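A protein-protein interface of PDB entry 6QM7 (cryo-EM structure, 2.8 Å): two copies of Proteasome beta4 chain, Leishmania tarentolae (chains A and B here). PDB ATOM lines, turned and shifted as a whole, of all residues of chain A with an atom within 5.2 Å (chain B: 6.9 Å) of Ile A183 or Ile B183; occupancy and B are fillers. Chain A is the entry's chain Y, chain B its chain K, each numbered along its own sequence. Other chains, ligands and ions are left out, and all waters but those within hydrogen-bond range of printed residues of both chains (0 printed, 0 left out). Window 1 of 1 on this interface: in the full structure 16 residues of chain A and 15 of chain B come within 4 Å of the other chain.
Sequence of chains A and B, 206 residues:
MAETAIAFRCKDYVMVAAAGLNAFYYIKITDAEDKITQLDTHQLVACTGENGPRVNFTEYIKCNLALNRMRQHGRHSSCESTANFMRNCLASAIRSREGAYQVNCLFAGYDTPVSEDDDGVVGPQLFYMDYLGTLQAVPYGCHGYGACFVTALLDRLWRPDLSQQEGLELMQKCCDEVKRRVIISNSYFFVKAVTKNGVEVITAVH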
ATOM      1  N   LEU A  21       4.951 -14.686  34.323  1.00  0.00           N
ATOM      2  CA  LEU A  21       4.719 -13.982  33.038  1.00  0.00           C
ATOM      3  C   LEU A  21       3.369 -13.264  33.031  1.00  0.00           C
ATOM      4  O   LEU A  21       2.350 -13.938  33.159  1.00  0.00           O
ATOM      5  CB  LEU A  21       4.756 -14.989  31.886  1.00  0.00           C
ATOM      6  CG  LEU A  21       4.479 -14.368  30.522  1.00  0.00           C
ATOM      7  CD1 LEU A  21       5.668 -13.558  30.073  1.00  0.00           C
ATOM      8  CD2 LEU A  21       4.142 -15.414  29.478  1.00  0.00           C
ATOM      9  N   ALA A  23       2.004 -10.706  29.917  1.00  0.00           N
ATOM     10  CA  ALA A  23       2.438 -10.445  28.530  1.00  0.00           C
ATOM     11  C   ALA A  23       1.401  -9.577  27.832  1.00  0.00           C
ATOM     12  O   ALA A  23       0.210  -9.663  28.182  1.00  0.00           O
ATOM     13  CB  ALA A  23       2.607 -11.751  27.814  1.00  0.00           C
ATOM     14  N   TYR A  25       0.602  -9.123  23.790  1.00  0.00           N
ATOM     15  CA  TYR A  25       1.011  -9.767  22.518  1.00  0.00           C
ATOM     16  C   TYR A  25       2.312 -10.513  22.823  1.00  0.00           C
ATOM     17  O   TYR A  25       2.243 -11.406  23.677  1.00  0.00           O
ATOM     18  CB  TYR A  25       1.105  -8.753  21.368  1.00  0.00           C
ATOM     19  CG  TYR A  25      -0.158  -8.014  20.977  1.00  0.00           C
ATOM     20  CD1 TYR A  25      -0.085  -6.945  20.089  1.00  0.00           C
ATOM     21  CD2 TYR A  25      -1.416  -8.340  21.487  1.00  0.00           C
ATOM     22  CE1 TYR A  25      -1.215  -6.234  19.704  1.00  0.00           C
ATOM     23  CE2 TYR A  25      -2.554  -7.633  21.116  1.00  0.00           C
ATOM     24  CZ  TYR A  25      -2.455  -6.579  20.221  1.00  0.00           C
ATOM     25  OH  TYR A  25      -3.570  -5.881  19.849  1.00  0.00           O
ATOM     26  N   TYR A  26       3.444 -10.106  22.245  1.00  0.00           N
ATOM     27  CA  TYR A  26       4.745 -10.821  22.358  1.00  0.00           C
ATOM     28  C   TYR A  26       5.677 -10.113  23.347  1.00  0.00           C
ATOM     29  O   TYR A  26       6.802 -10.569  23.496  1.00  0.00           O
ATOM     30  CB  TYR A  26       5.410 -10.975  20.985  1.00  0.00           C
ATOM     31  CG  TYR A  26       5.663  -9.688  20.241  1.00  0.00           C
ATOM     32  CD1 TYR A  26       6.774  -8.901  20.510  1.00  0.00           C
ATOM     33  CD2 TYR A  26       4.789  -9.251  19.260  1.00  0.00           C
ATOM     34  CE1 TYR A  26       7.005  -7.711  19.833  1.00  0.00           C
ATOM     35  CE2 TYR A  26       5.007  -8.064  18.572  1.00  0.00           C
ATOM     36  CZ  TYR A  26       6.114  -7.283  18.863  1.00  0.00           C
ATOM     37  OH  TYR A  26       6.322  -6.118  18.181  1.00  0.00           O
ATOM     38  N   ILE A  27       5.220  -9.063  24.023  1.00  0.00           N
ATOM     39  CA  ILE A  27       6.044  -8.220  24.935  1.00  0.00           C
ATOM     40  C   ILE A  27       5.818  -8.694  26.370  1.00  0.00           C
ATOM     41  O   ILE A  27       4.682  -8.546  26.834  1.00  0.00           O
ATOM     42  CB  ILE A  27       5.662  -6.737  24.782  1.00  0.00           C
ATOM     43  CG1 ILE A  27       5.592  -6.316  23.314  1.00  0.00           C
ATOM     44  CG2 ILE A  27       6.614  -5.855  25.578  1.00  0.00           C
ATOM     45  CD1 ILE A  27       5.184  -4.872  23.111  1.00  0.00           C
ATOM     46  N   LYS A  28       6.843  -9.227  27.043  1.00  0.00           N
ATOM     47  CA  LYS A  28       6.815  -9.482  28.508  1.00  0.00           C
ATOM     48  C   LYS A  28       6.689  -8.145  29.245  1.00  0.00           C
ATOM     49  O   LYS A  28       7.675  -7.398  29.333  1.00  0.00           O
ATOM     50  CB  LYS A  28       8.091 -10.152  29.029  1.00  0.00           C
ATOM     51  CG  LYS A  28       8.231 -11.634  28.733  1.00  0.00           C
ATOM     52  CD  LYS A  28       9.097 -12.371  29.741  1.00  0.00           C
ATOM     53  CE  LYS A  28      10.418 -12.861  29.180  1.00  0.00           C
ATOM     54  NZ  LYS A  28      11.298 -13.321  30.282  1.00  0.00           N
ATOM     55  N   ARG A 181      10.955 -26.641  27.673  1.00  0.00           N
ATOM     56  CA  ARG A 181      10.101 -27.261  26.630  1.00  0.00           C
ATOM     57  C   ARG A 181       9.009 -26.340  26.094  1.00  0.00           C
ATOM     58  O   ARG A 181       8.644 -26.540  24.942  1.00  0.00           O
ATOM     59  CB  ARG A 181       9.460 -28.533  27.178  1.00  0.00           C
ATOM     60  CG  ARG A 181       9.653 -29.711  26.243  1.00  0.00           C
ATOM     61  CD  ARG A 181      11.106 -30.122  26.188  1.00  0.00           C
ATOM     62  NE  ARG A 181      11.710 -30.114  24.868  1.00  0.00           N
ATOM     63  CZ  ARG A 181      12.845 -30.736  24.566  1.00  0.00           C
ATOM     64  NH1 ARG A 181      13.325 -30.678  23.339  1.00  0.00           N
ATOM     65  NH2 ARG A 181      13.507 -31.423  25.476  1.00  0.00           N
ATOM     66  N   VAL A 182       8.467 -25.414  26.872  1.00  0.00           N
ATOM     67  CA  VAL A 182       7.445 -24.469  26.351  1.00  0.00           C
ATOM     68  C   VAL A 182       8.155 -23.243  25.796  1.00  0.00           C
ATOM     69  O   VAL A 182       9.107 -22.769  26.450  1.00  0.00           O
ATOM     70  CB  VAL A 182       6.434 -24.097  27.435  1.00  0.00           C
ATOM     71  CG1 VAL A 182       5.412 -23.103  26.912  1.00  0.00           C
ATOM     72  CG2 VAL A 182       5.749 -25.346  27.979  1.00  0.00           C
ATOM     73  N   ILE A 183       7.733 -22.771  24.619  1.00  0.00           N
ATOM     74  CA  ILE A 183       8.423 -21.661  23.896  1.00  0.00           C
ATOM     75  C   ILE A 183       8.108 -20.367  24.631  1.00  0.00           C
ATOM     76  O   ILE A 183       8.975 -19.495  24.639  1.00  0.00           O
ATOM     77  CB  ILE A 183       8.070 -21.557  22.395  1.00  0.00           C
ATOM     78  CG1 ILE A 183       6.622 -21.129  22.139  1.00  0.00           C
ATOM     79  CG2 ILE A 183       8.412 -22.853  21.676  1.00  0.00           C
ATOM     80  CD1 ILE A 183       6.373 -20.741  20.695  1.00  0.00           C
ATOM     81  N   ILE A 184       6.919 -20.262  25.214  1.00  0.00           N
ATOM     82  CA  ILE A 184       6.542 -19.093  26.050  1.00  0.00           C
ATOM     83  C   ILE A 184       7.442 -19.103  27.282  1.00  0.00           C
ATOM     84  O   ILE A 184       7.411 -20.096  28.030  1.00  0.00           O
ATOM     85  CB  ILE A 184       5.059 -19.096  26.440  1.00  0.00           C
ATOM     86  CG1 ILE A 184       4.115 -19.139  25.230  1.00  0.00           C
ATOM     87  CG2 ILE A 184       4.780 -17.901  27.333  1.00  0.00           C
ATOM     88  CD1 ILE A 184       4.244 -17.967  24.270  1.00  0.00           C
ATOM     89  N   SER A 185       8.209 -18.025  27.457  1.00  0.00           N
ATOM     90  CA  SER A 185       9.232 -17.843  28.512  1.00  0.00           C
ATOM     91  C   SER A 185       8.515 -17.684  29.853  1.00  0.00           C
ATOM     92  O   SER A 185       8.039 -16.564  30.152  1.00  0.00           O
ATOM     93  CB  SER A 185      10.145 -16.679  28.215  1.00  0.00           C
ATOM     94  OG  SER A 185      11.238 -16.661  29.123  1.00  0.00           O
ATOM     95  N   ALA B   2       9.213 -15.402  15.937  1.00  0.00           N
ATOM     96  CA  ALA B   2       9.596 -16.145  17.164  1.00  0.00           C
ATOM     97  C   ALA B   2      11.112 -16.057  17.358  1.00  0.00           C
ATOM     98  O   ALA B   2      11.549 -15.656  18.454  1.00  0.00           O
ATOM     99  CB  ALA B   2       9.138 -17.584  17.080  1.00  0.00           C
ATOM    100  N   LEU B  21      16.201 -21.086  18.978  1.00  0.00           N
ATOM    101  CA  LEU B  21      14.863 -21.712  19.104  1.00  0.00           C
ATOM    102  C   LEU B  21      14.398 -22.279  17.768  1.00  0.00           C
ATOM    103  O   LEU B  21      14.224 -21.493  16.838  1.00  0.00           O
ATOM    104  CB  LEU B  21      13.853 -20.668  19.563  1.00  0.00           C
ATOM    105  CG  LEU B  21      12.413 -21.174  19.606  1.00  0.00           C
ATOM    106  CD1 LEU B  21      12.245 -22.161  20.736  1.00  0.00           C
ATOM    107  CD2 LEU B  21      11.420 -20.030  19.744  1.00  0.00           C
ATOM    108  N   ASN B  22      14.191 -23.594  17.716  1.00  0.00           N
ATOM    109  CA  ASN B  22      13.271 -24.276  16.773  1.00  0.00           C
ATOM    110  C   ASN B  22      12.080 -24.731  17.611  1.00  0.00           C
ATOM    111  O   ASN B  22      12.304 -25.265  18.694  1.00  0.00           O
ATOM    112  CB  ASN B  22      13.946 -25.442  16.052  1.00  0.00           C
ATOM    113  CG  ASN B  22      13.102 -26.022  14.934  1.00  0.00           C
ATOM    114  OD1 ASN B  22      11.993 -26.497  15.166  1.00  0.00           O
ATOM    115  ND2 ASN B  22      13.630 -26.022  13.718  1.00  0.00           N
ATOM    116  N   ALA B  23      10.869 -24.500  17.128  1.00  0.00           N
ATOM    117  CA  ALA B  23       9.613 -24.694  17.881  1.00  0.00           C
ATOM    118  C   ALA B  23       8.610 -25.434  17.006  1.00  0.00           C
ATOM    119  O   ALA B  23       8.669 -25.304  15.773  1.00  0.00           O
ATOM    120  CB  ALA B  23       9.052 -23.357  18.298  1.00  0.00           C
ATOM    121  N   PHE B  24       7.708 -26.165  17.641  1.00  0.00           N
ATOM    122  CA  PHE B  24       6.558 -26.817  16.988  1.00  0.00           C
ATOM    123  C   PHE B  24       5.321 -26.435  17.787  1.00  0.00           C
ATOM    124  O   PHE B  24       5.154 -26.971  18.888  1.00  0.00           O
ATOM    125  CB  PHE B  24       6.756 -28.328  16.922  1.00  0.00           C
ATOM    126  CG  PHE B  24       5.563 -29.033  16.346  1.00  0.00           C
ATOM    127  CD1 PHE B  24       5.343 -29.041  14.980  1.00  0.00           C
ATOM    128  CD2 PHE B  24       4.624 -29.623  17.174  1.00  0.00           C
ATOM    129  CE1 PHE B  24       4.214 -29.650  14.457  1.00  0.00           C
ATOM    130  CE2 PHE B  24       3.492 -30.223  16.651  1.00  0.00           C
ATOM    131  CZ  PHE B  24       3.293 -30.243  15.293  1.00  0.00           C
ATOM    132  N   TYR B  25       4.485 -25.557  17.243  1.00  0.00           N
ATOM    133  CA  TYR B  25       3.417 -24.861  17.996  1.00  0.00           C
ATOM    134  C   TYR B  25       4.103 -24.238  19.211  1.00  0.00           C
ATOM    135  O   TYR B  25       4.960 -23.370  18.984  1.00  0.00           O
ATOM    136  CB  TYR B  25       2.255 -25.804  18.332  1.00  0.00           C
ATOM    137  CG  TYR B  25       1.492 -26.411  17.173  1.00  0.00           C
ATOM    138  CD1 TYR B  25       0.566 -27.426  17.410  1.00  0.00           C
ATOM    139  CD2 TYR B  25       1.681 -26.010  15.851  1.00  0.00           C
ATOM    140  CE1 TYR B  25      -0.154 -28.012  16.378  1.00  0.00           C
ATOM    141  CE2 TYR B  25       0.971 -26.591  14.807  1.00  0.00           C
ATOM    142  CZ  TYR B  25       0.049 -27.594  15.070  1.00  0.00           C
ATOM    143  OH  TYR B  25      -0.651 -28.169  14.046  1.00  0.00           O
ATOM    144  N   TYR B  26       3.823 -24.726  20.419  1.00  0.00           N
ATOM    145  CA  TYR B  26       4.328 -24.155  21.690  1.00  0.00           C
ATOM    146  C   TYR B  26       5.462 -25.003  22.286  1.00  0.00           C
ATOM    147  O   TYR B  26       5.918 -24.658  23.366  1.00  0.00           O
ATOM    148  CB  TYR B  26       3.179 -23.987  22.681  1.00  0.00           C
ATOM    149  CG  TYR B  26       2.435 -25.244  23.041  1.00  0.00           C
ATOM    150  CD1 TYR B  26       2.931 -26.147  23.975  1.00  0.00           C
ATOM    151  CD2 TYR B  26       1.194 -25.509  22.481  1.00  0.00           C
ATOM    152  CE1 TYR B  26       2.224 -27.291  24.322  1.00  0.00           C
ATOM    153  CE2 TYR B  26       0.473 -26.647  22.818  1.00  0.00           C
ATOM    154  CZ  TYR B  26       0.992 -27.542  23.737  1.00  0.00           C
ATOM    155  OH  TYR B  26       0.272 -28.661  24.042  1.00  0.00           O
ATOM    156  N   ILE B  27       5.922 -26.046  21.604  1.00  0.00           N
ATOM    157  CA  ILE B  27       6.914 -27.022  22.136  1.00  0.00           C
ATOM    158  C   ILE B  27       8.288 -26.637  21.588  1.00  0.00           C
ATOM    159  O   ILE B  27       8.441 -26.650  20.373  1.00  0.00           O
ATOM    160  CB  ILE B  27       6.538 -28.466  21.746  1.00  0.00           C
ATOM    161  CG1 ILE B  27       5.064 -28.780  22.016  1.00  0.00           C
ATOM    162  CG2 ILE B  27       7.455 -29.467  22.434  1.00  0.00           C
ATOM    163  CD1 ILE B  27       4.618 -30.117  21.475  1.00  0.00           C
ATOM    164  N   LYS B  28       9.234 -26.272  22.447  1.00  0.00           N
ATOM    165  CA  LYS B  28      10.638 -26.065  22.035  1.00  0.00           C
ATOM    166  C   LYS B  28      11.197 -27.421  21.635  1.00  0.00           C
ATOM    167  O   LYS B  28      11.415 -28.260  22.530  1.00  0.00           O
ATOM    168  CB  LYS B  28      11.539 -25.530  23.150  1.00  0.00           C
ATOM    169  CG  LYS B  28      11.390 -24.059  23.480  1.00  0.00           C
ATOM    170  CD  LYS B  28      12.658 -23.461  24.057  1.00  0.00           C
ATOM    171  CE  LYS B  28      12.568 -23.163  25.538  1.00  0.00           C
ATOM    172  NZ  LYS B  28      13.910 -22.816  26.065  1.00  0.00           N
ATOM    173  N   ILE B  29      11.413 -27.619  20.344  1.00  0.00           N
ATOM    174  CA  ILE B  29      12.068 -28.841  19.810  1.00  0.00           C
ATOM    175  C   ILE B  29      13.519 -28.798  20.255  1.00  0.00           C
ATOM    176  O   ILE B  29      14.069 -29.848  20.586  1.00  0.00           O
ATOM    177  CB  ILE B  29      11.934 -28.888  18.287  1.00  0.00           C
ATOM    178  CG1 ILE B  29      10.467 -29.036  17.880  1.00  0.00           C
ATOM    179  CG2 ILE B  29      12.816 -29.976  17.703  1.00  0.00           C
ATOM    180  CD1 ILE B  29      10.218 -28.826  16.391  1.00  0.00           C
ATOM    181  N   TYR B 145      10.568 -10.787  16.790  1.00  0.00           N
ATOM    182  CA  TYR B 145       9.804 -10.054  17.822  1.00  0.00           C
ATOM    183  C   TYR B 145      10.750  -9.113  18.564  1.00  0.00           C
ATOM    184  O   TYR B 145      10.334  -7.989  18.891  1.00  0.00           O
ATOM    185  CB  TYR B 145       9.133 -11.054  18.761  1.00  0.00           C
ATOM    186  CG  TYR B 145       7.935 -11.787  18.203  1.00  0.00           C
ATOM    187  CD1 TYR B 145       7.007 -11.159  17.380  1.00  0.00           C
ATOM    188  CD2 TYR B 145       7.692 -13.101  18.566  1.00  0.00           C
ATOM    189  CE1 TYR B 145       5.889 -11.830  16.907  1.00  0.00           C
ATOM    190  CE2 TYR B 145       6.585 -13.790  18.094  1.00  0.00           C
ATOM    191  CZ  TYR B 145       5.676 -13.155  17.261  1.00  0.00           C
ATOM    192  OH  TYR B 145       4.582 -13.834  16.794  1.00  0.00           O
ATOM    193  N   VAL B 178      16.427  -9.130  24.354  1.00  0.00           N
ATOM    194  CA  VAL B 178      15.408 -10.010  23.718  1.00  0.00           C
ATOM    195  C   VAL B 178      14.852 -10.950  24.795  1.00  0.00           C
ATOM    196  O   VAL B 178      13.620 -11.101  24.841  1.00  0.00           O
ATOM    197  CB  VAL B 178      15.990 -10.768  22.512  1.00  0.00           C
ATOM    198  CG1 VAL B 178      15.041 -11.823  21.963  1.00  0.00           C
ATOM    199  CG2 VAL B 178      16.387  -9.787  21.422  1.00  0.00           C
ATOM    200  N   LYS B 179      15.719 -11.553  25.616  1.00  0.00           N
ATOM    201  CA  LYS B 179      15.334 -12.555  26.644  1.00  0.00           C
ATOM    202  C   LYS B 179      14.442 -11.877  27.683  1.00  0.00           C
ATOM    203  O   LYS B 179      13.409 -12.465  28.041  1.00  0.00           O
ATOM    204  CB  LYS B 179      16.554 -13.174  27.328  1.00  0.00           C
ATOM    205  CG  LYS B 179      17.504 -13.976  26.436  1.00  0.00           C
ATOM    206  CD  LYS B 179      18.974 -13.851  26.882  1.00  0.00           C
ATOM    207  CE  LYS B 179      19.776 -15.138  26.911  1.00  0.00           C
ATOM    208  NZ  LYS B 179      20.249 -15.504  25.560  1.00  0.00           N
ATOM    209  N   ARG B 180      14.813 -10.669  28.103  1.00  0.00           N
ATOM    210  CA  ARG B 180      14.093  -9.837  29.108  1.00  0.00           C
ATOM    211  C   ARG B 180      12.662  -9.529  28.657  1.00  0.00           C
ATOM    212  O   ARG B 180      11.788  -9.450  29.530  1.00  0.00           O
ATOM    213  CB  ARG B 180      14.841  -8.512  29.309  1.00  0.00           C
ATOM    214  CG  ARG B 180      14.269  -7.610  30.398  1.00  0.00           C
ATOM    215  CD  ARG B 180      15.222  -6.513  30.847  1.00  0.00           C
ATOM    216  NE  ARG B 180      16.586  -6.993  31.098  1.00  0.00           N
ATOM    217  CZ  ARG B 180      17.682  -6.690  30.388  1.00  0.00           C
ATOM    218  NH1 ARG B 180      17.638  -5.875  29.345  1.00  0.00           N
ATOM    219  NH2 ARG B 180      18.846  -7.215  30.736  1.00  0.00           N
ATOM    220  N   ARG B 181      12.439  -9.317  27.361  1.00  0.00           N
ATOM    221  CA  ARG B 181      11.254  -8.572  26.881  1.00  0.00           C
ATOM    222  C   ARG B 181      10.354  -9.373  25.944  1.00  0.00           C
ATOM    223  O   ARG B 181       9.139  -9.095  25.953  1.00  0.00           O
ATOM    224  CB  ARG B 181      11.697  -7.282  26.195  1.00  0.00           C
ATOM    225  CG  ARG B 181      10.898  -6.083  26.683  1.00  0.00           C
ATOM    226  CD  ARG B 181      11.257  -5.774  28.121  1.00  0.00           C
ATOM    227  NE  ARG B 181      10.129  -5.693  29.023  1.00  0.00           N
ATOM    228  CZ  ARG B 181      10.196  -5.155  30.229  1.00  0.00           C
ATOM    229  NH1 ARG B 181       9.118  -5.103  30.992  1.00  0.00           N
ATOM    230  NH2 ARG B 181      11.333  -4.667  30.687  1.00  0.00           N
ATOM    231  N   VAL B 182      10.897 -10.263  25.125  1.00  0.00           N
ATOM    232  CA  VAL B 182      10.064 -11.085  24.204  1.00  0.00           C
ATOM    233  C   VAL B 182       9.545 -12.293  24.983  1.00  0.00           C
ATOM    234  O   VAL B 182      10.339 -12.873  25.763  1.00  0.00           O
ATOM    235  CB  VAL B 182      10.850 -11.482  22.947  1.00  0.00           C
ATOM    236  CG1 VAL B 182      10.004 -12.318  22.005  1.00  0.00           C
ATOM    237  CG2 VAL B 182      11.377 -10.240  22.239  1.00  0.00           C
ATOM    238  N   ILE B 183       8.270 -12.651  24.803  1.00  0.00           N
ATOM    239  CA  ILE B 183       7.656 -13.769  25.575  1.00  0.00           C
ATOM    240  C   ILE B 183       8.147 -15.075  24.988  1.00  0.00           C
ATOM    241  O   ILE B 183       8.273 -16.014  25.760  1.00  0.00           O
ATOM    242  CB  ILE B 183       6.120 -13.744  25.659  1.00  0.00           C
ATOM    243  CG1 ILE B 183       5.416 -13.996  24.330  1.00  0.00           C
ATOM    244  CG2 ILE B 183       5.656 -12.450  26.291  1.00  0.00           C
ATOM    245  CD1 ILE B 183       3.925 -14.190  24.508  1.00  0.00           C
ATOM    246  N   ILE B 184       8.411 -15.119  23.689  1.00  0.00           N
ATOM    247  CA  ILE B 184       9.018 -16.319  23.047  1.00  0.00           C
ATOM    248  C   ILE B 184      10.426 -16.484  23.609  1.00  0.00           C
ATOM    249  O   ILE B 184      11.225 -15.557  23.442  1.00  0.00           O
ATOM    250  CB  ILE B 184       9.036 -16.204  21.517  1.00  0.00           C
ATOM    251  CG1 ILE B 184       7.647 -15.932  20.923  1.00  0.00           C
ATOM    252  CG2 ILE B 184       9.674 -17.446  20.924  1.00  0.00           C
ATOM    253  CD1 ILE B 184       6.598 -16.958  21.280  1.00  0.00           C
ATOM    254  N   SER B 185      10.692 -17.621  24.249  1.00  0.00           N
ATOM    255  CA  SER B 185      11.979 -17.968  24.905  1.00  0.00           C
ATOM    256  C   SER B 185      13.070 -18.125  23.840  1.00  0.00           C
ATOM    257  O   SER B 185      13.114 -19.194  23.180  1.00  0.00           O
ATOM    258  CB  SER B 185      11.858 -19.209  25.770  1.00  0.00           C
ATOM    259  OG  SER B 185      13.024 -19.384  26.570  1.00  0.00           O
ATOM    260  N   ASN B 186      13.885 -17.070  23.677  1.00  0.00           N
ATOM    261  CA  ASN B 186      15.125 -17.050  22.859  1.00  0.00           C
ATOM    262  C   ASN B 186      16.281 -17.097  23.847  1.00  0.00           C
ATOM    263  O   ASN B 186      16.948 -16.087  24.032  1.00  0.00           O
ATOM    264  CB  ASN B 186      15.172 -15.844  21.916  1.00  0.00           C
ATOM    265  CG  ASN B 186      14.122 -15.892  20.823  1.00  0.00           C
ATOM    266  OD1 ASN B 186      13.936 -14.920  20.090  1.00  0.00           O
ATOM    267  ND2 ASN B 186      13.419 -17.010  20.704  1.00  0.00           N
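The backbone carbonyl oxygen (O) of Asn B22 sits at hydrogen-bond distance from the backbone NH (N) of Ile B29.
Printed residues of chain B within 4 Å of Ile A183: Ala B23, Tyr B25, Tyr B26, Ile B27, Lys B28, Ile B183, Ile B184 and Ser B185.
Of the printed residues of chain A, Ile B183 touches Leu A21, Ala A23, Tyr A25, Tyr A26, Ile A27, Lys A28, Ile A183, Ile A184 and Ser A185.
Of the printed residues of chain A, Arg B180 touches Lys A28 (3.7 Å).
Of the printed residues of chain B, Tyr A26 touches Tyr B145, Arg B181, Val B182 and Ile B183.
Of the printed residues of chain B, Ser A185 touches Ile B183 (2.6 Å) and Ser B185 (3.9 Å).
Of the printed residues of chain B, Ile A27 touches Arg B181 (3.4 Å) and Ile B183 (3.8 Å).
Of the printed residues of chain B, Arg A181 touches Tyr B26, Ile B27, Lys B28 and Ile B29.
The nearest printed residue of chain B that does not touch Ile A183 is Leu B21 (4.01 Å).
The nearest printed residue of chain A that does not touch Lys B28 is Ile A184 (6.1 Å).
O of Tyr B26 is in hydrogen-bond range of N of Ile A183, 2.9 Å away.
N of Lys B28 lies within hydrogen-bond range of O of Arg A181, at 2.6 Å.
NH1 of Arg A181 sits at hydrogen-bond distance from O of Ile B29, at 3.0 Å.
The backbone carbonyl oxygen (O) of Lys B179 lies within hydrogen-bond range of the side-chain amino group (NZ) of Lys A28.
The backbone carbonyl oxygen of Arg B181 lies within hydrogen-bond range of the backbone NH of Lys A28.
O of Tyr A26 is in hydrogen-bond range of N of Ile B183.
The backbone NH (N) of Ser A185 sits at hydrogen-bond distance from the backbone carbonyl oxygen (O) of Ile B183 (2.6 Å).
N of Ser B185 sits at hydrogen-bond distance from O of Ile A183, 2.6 Å away.
CG2 of Ile B183 touches CD1 of Leu A21 (3.9 Å).
Tyr A26 touches Arg B181.
Ile B183 touches Lys A28 (CG2 to N, 3.5 Å).
O of Tyr B26 touches O of Arg A181, at 3.7 Å.
O of Tyr B26 touches CA of Val A182 (3.4 Å).
Ile A183 touches Tyr B25.
Ile A183 touches Ile B27 (CG2 to C, 3.8 Å).
Ile B183 touches Ile A183.
O of Ile B183 touches C of Ile A184, 3.5 Å away.
Ile B184 touches Ile A184 (CD1 to CD1, 3.9 Å).
Of the 20 printed residues of chain B, 14 touch a printed residue of chain A.
Printed residues of chain B that touch a printed residue of chain A: Ala B23, Tyr B25, Tyr B26, Ile B27, Lys B28, Ile B29, Tyr B145, Lys B179, Arg B180, Arg B181, Val B182, Ile B183, Ile B184 and Ser B185.
Printed residues of chain A that touch a printed residue of chain B: Leu A21, Ala A23, Tyr A25, Tyr A26, Ile A27, Lys A28, Arg A181, Val A182, Ile A183, Ile A184 and Ser A185.
Hydrophobic or aromatic side chains of chain A that line the printed part of chain B: Leu A21, Ala A23, Tyr A26, Val A182, Ile A183 and Ile A184.
Along chain A the printed residues that touch a printed residue of chain B span positions 21 to 185.
Among the printed residues, no Asp or Glu carboxylate lies within 4 Å of a Lys or Arg side-chain nitrogen of the other chain.
Ala A23 touches Ile B183, and with the chains exchanged Ile A183 touches Ala B23.
Lys A28 touches Val B182, and with the chains exchanged Val A182 touches Lys B28.
Ile B184 touches its own counterpart, Ile A184.
Ser A185 touches its own counterpart, Ser B185.
11 positions are printed for both chains.
Of the 32 pairs that touch across the chains among the printed residues, 27 have their exchanged pair printed and touching as well.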
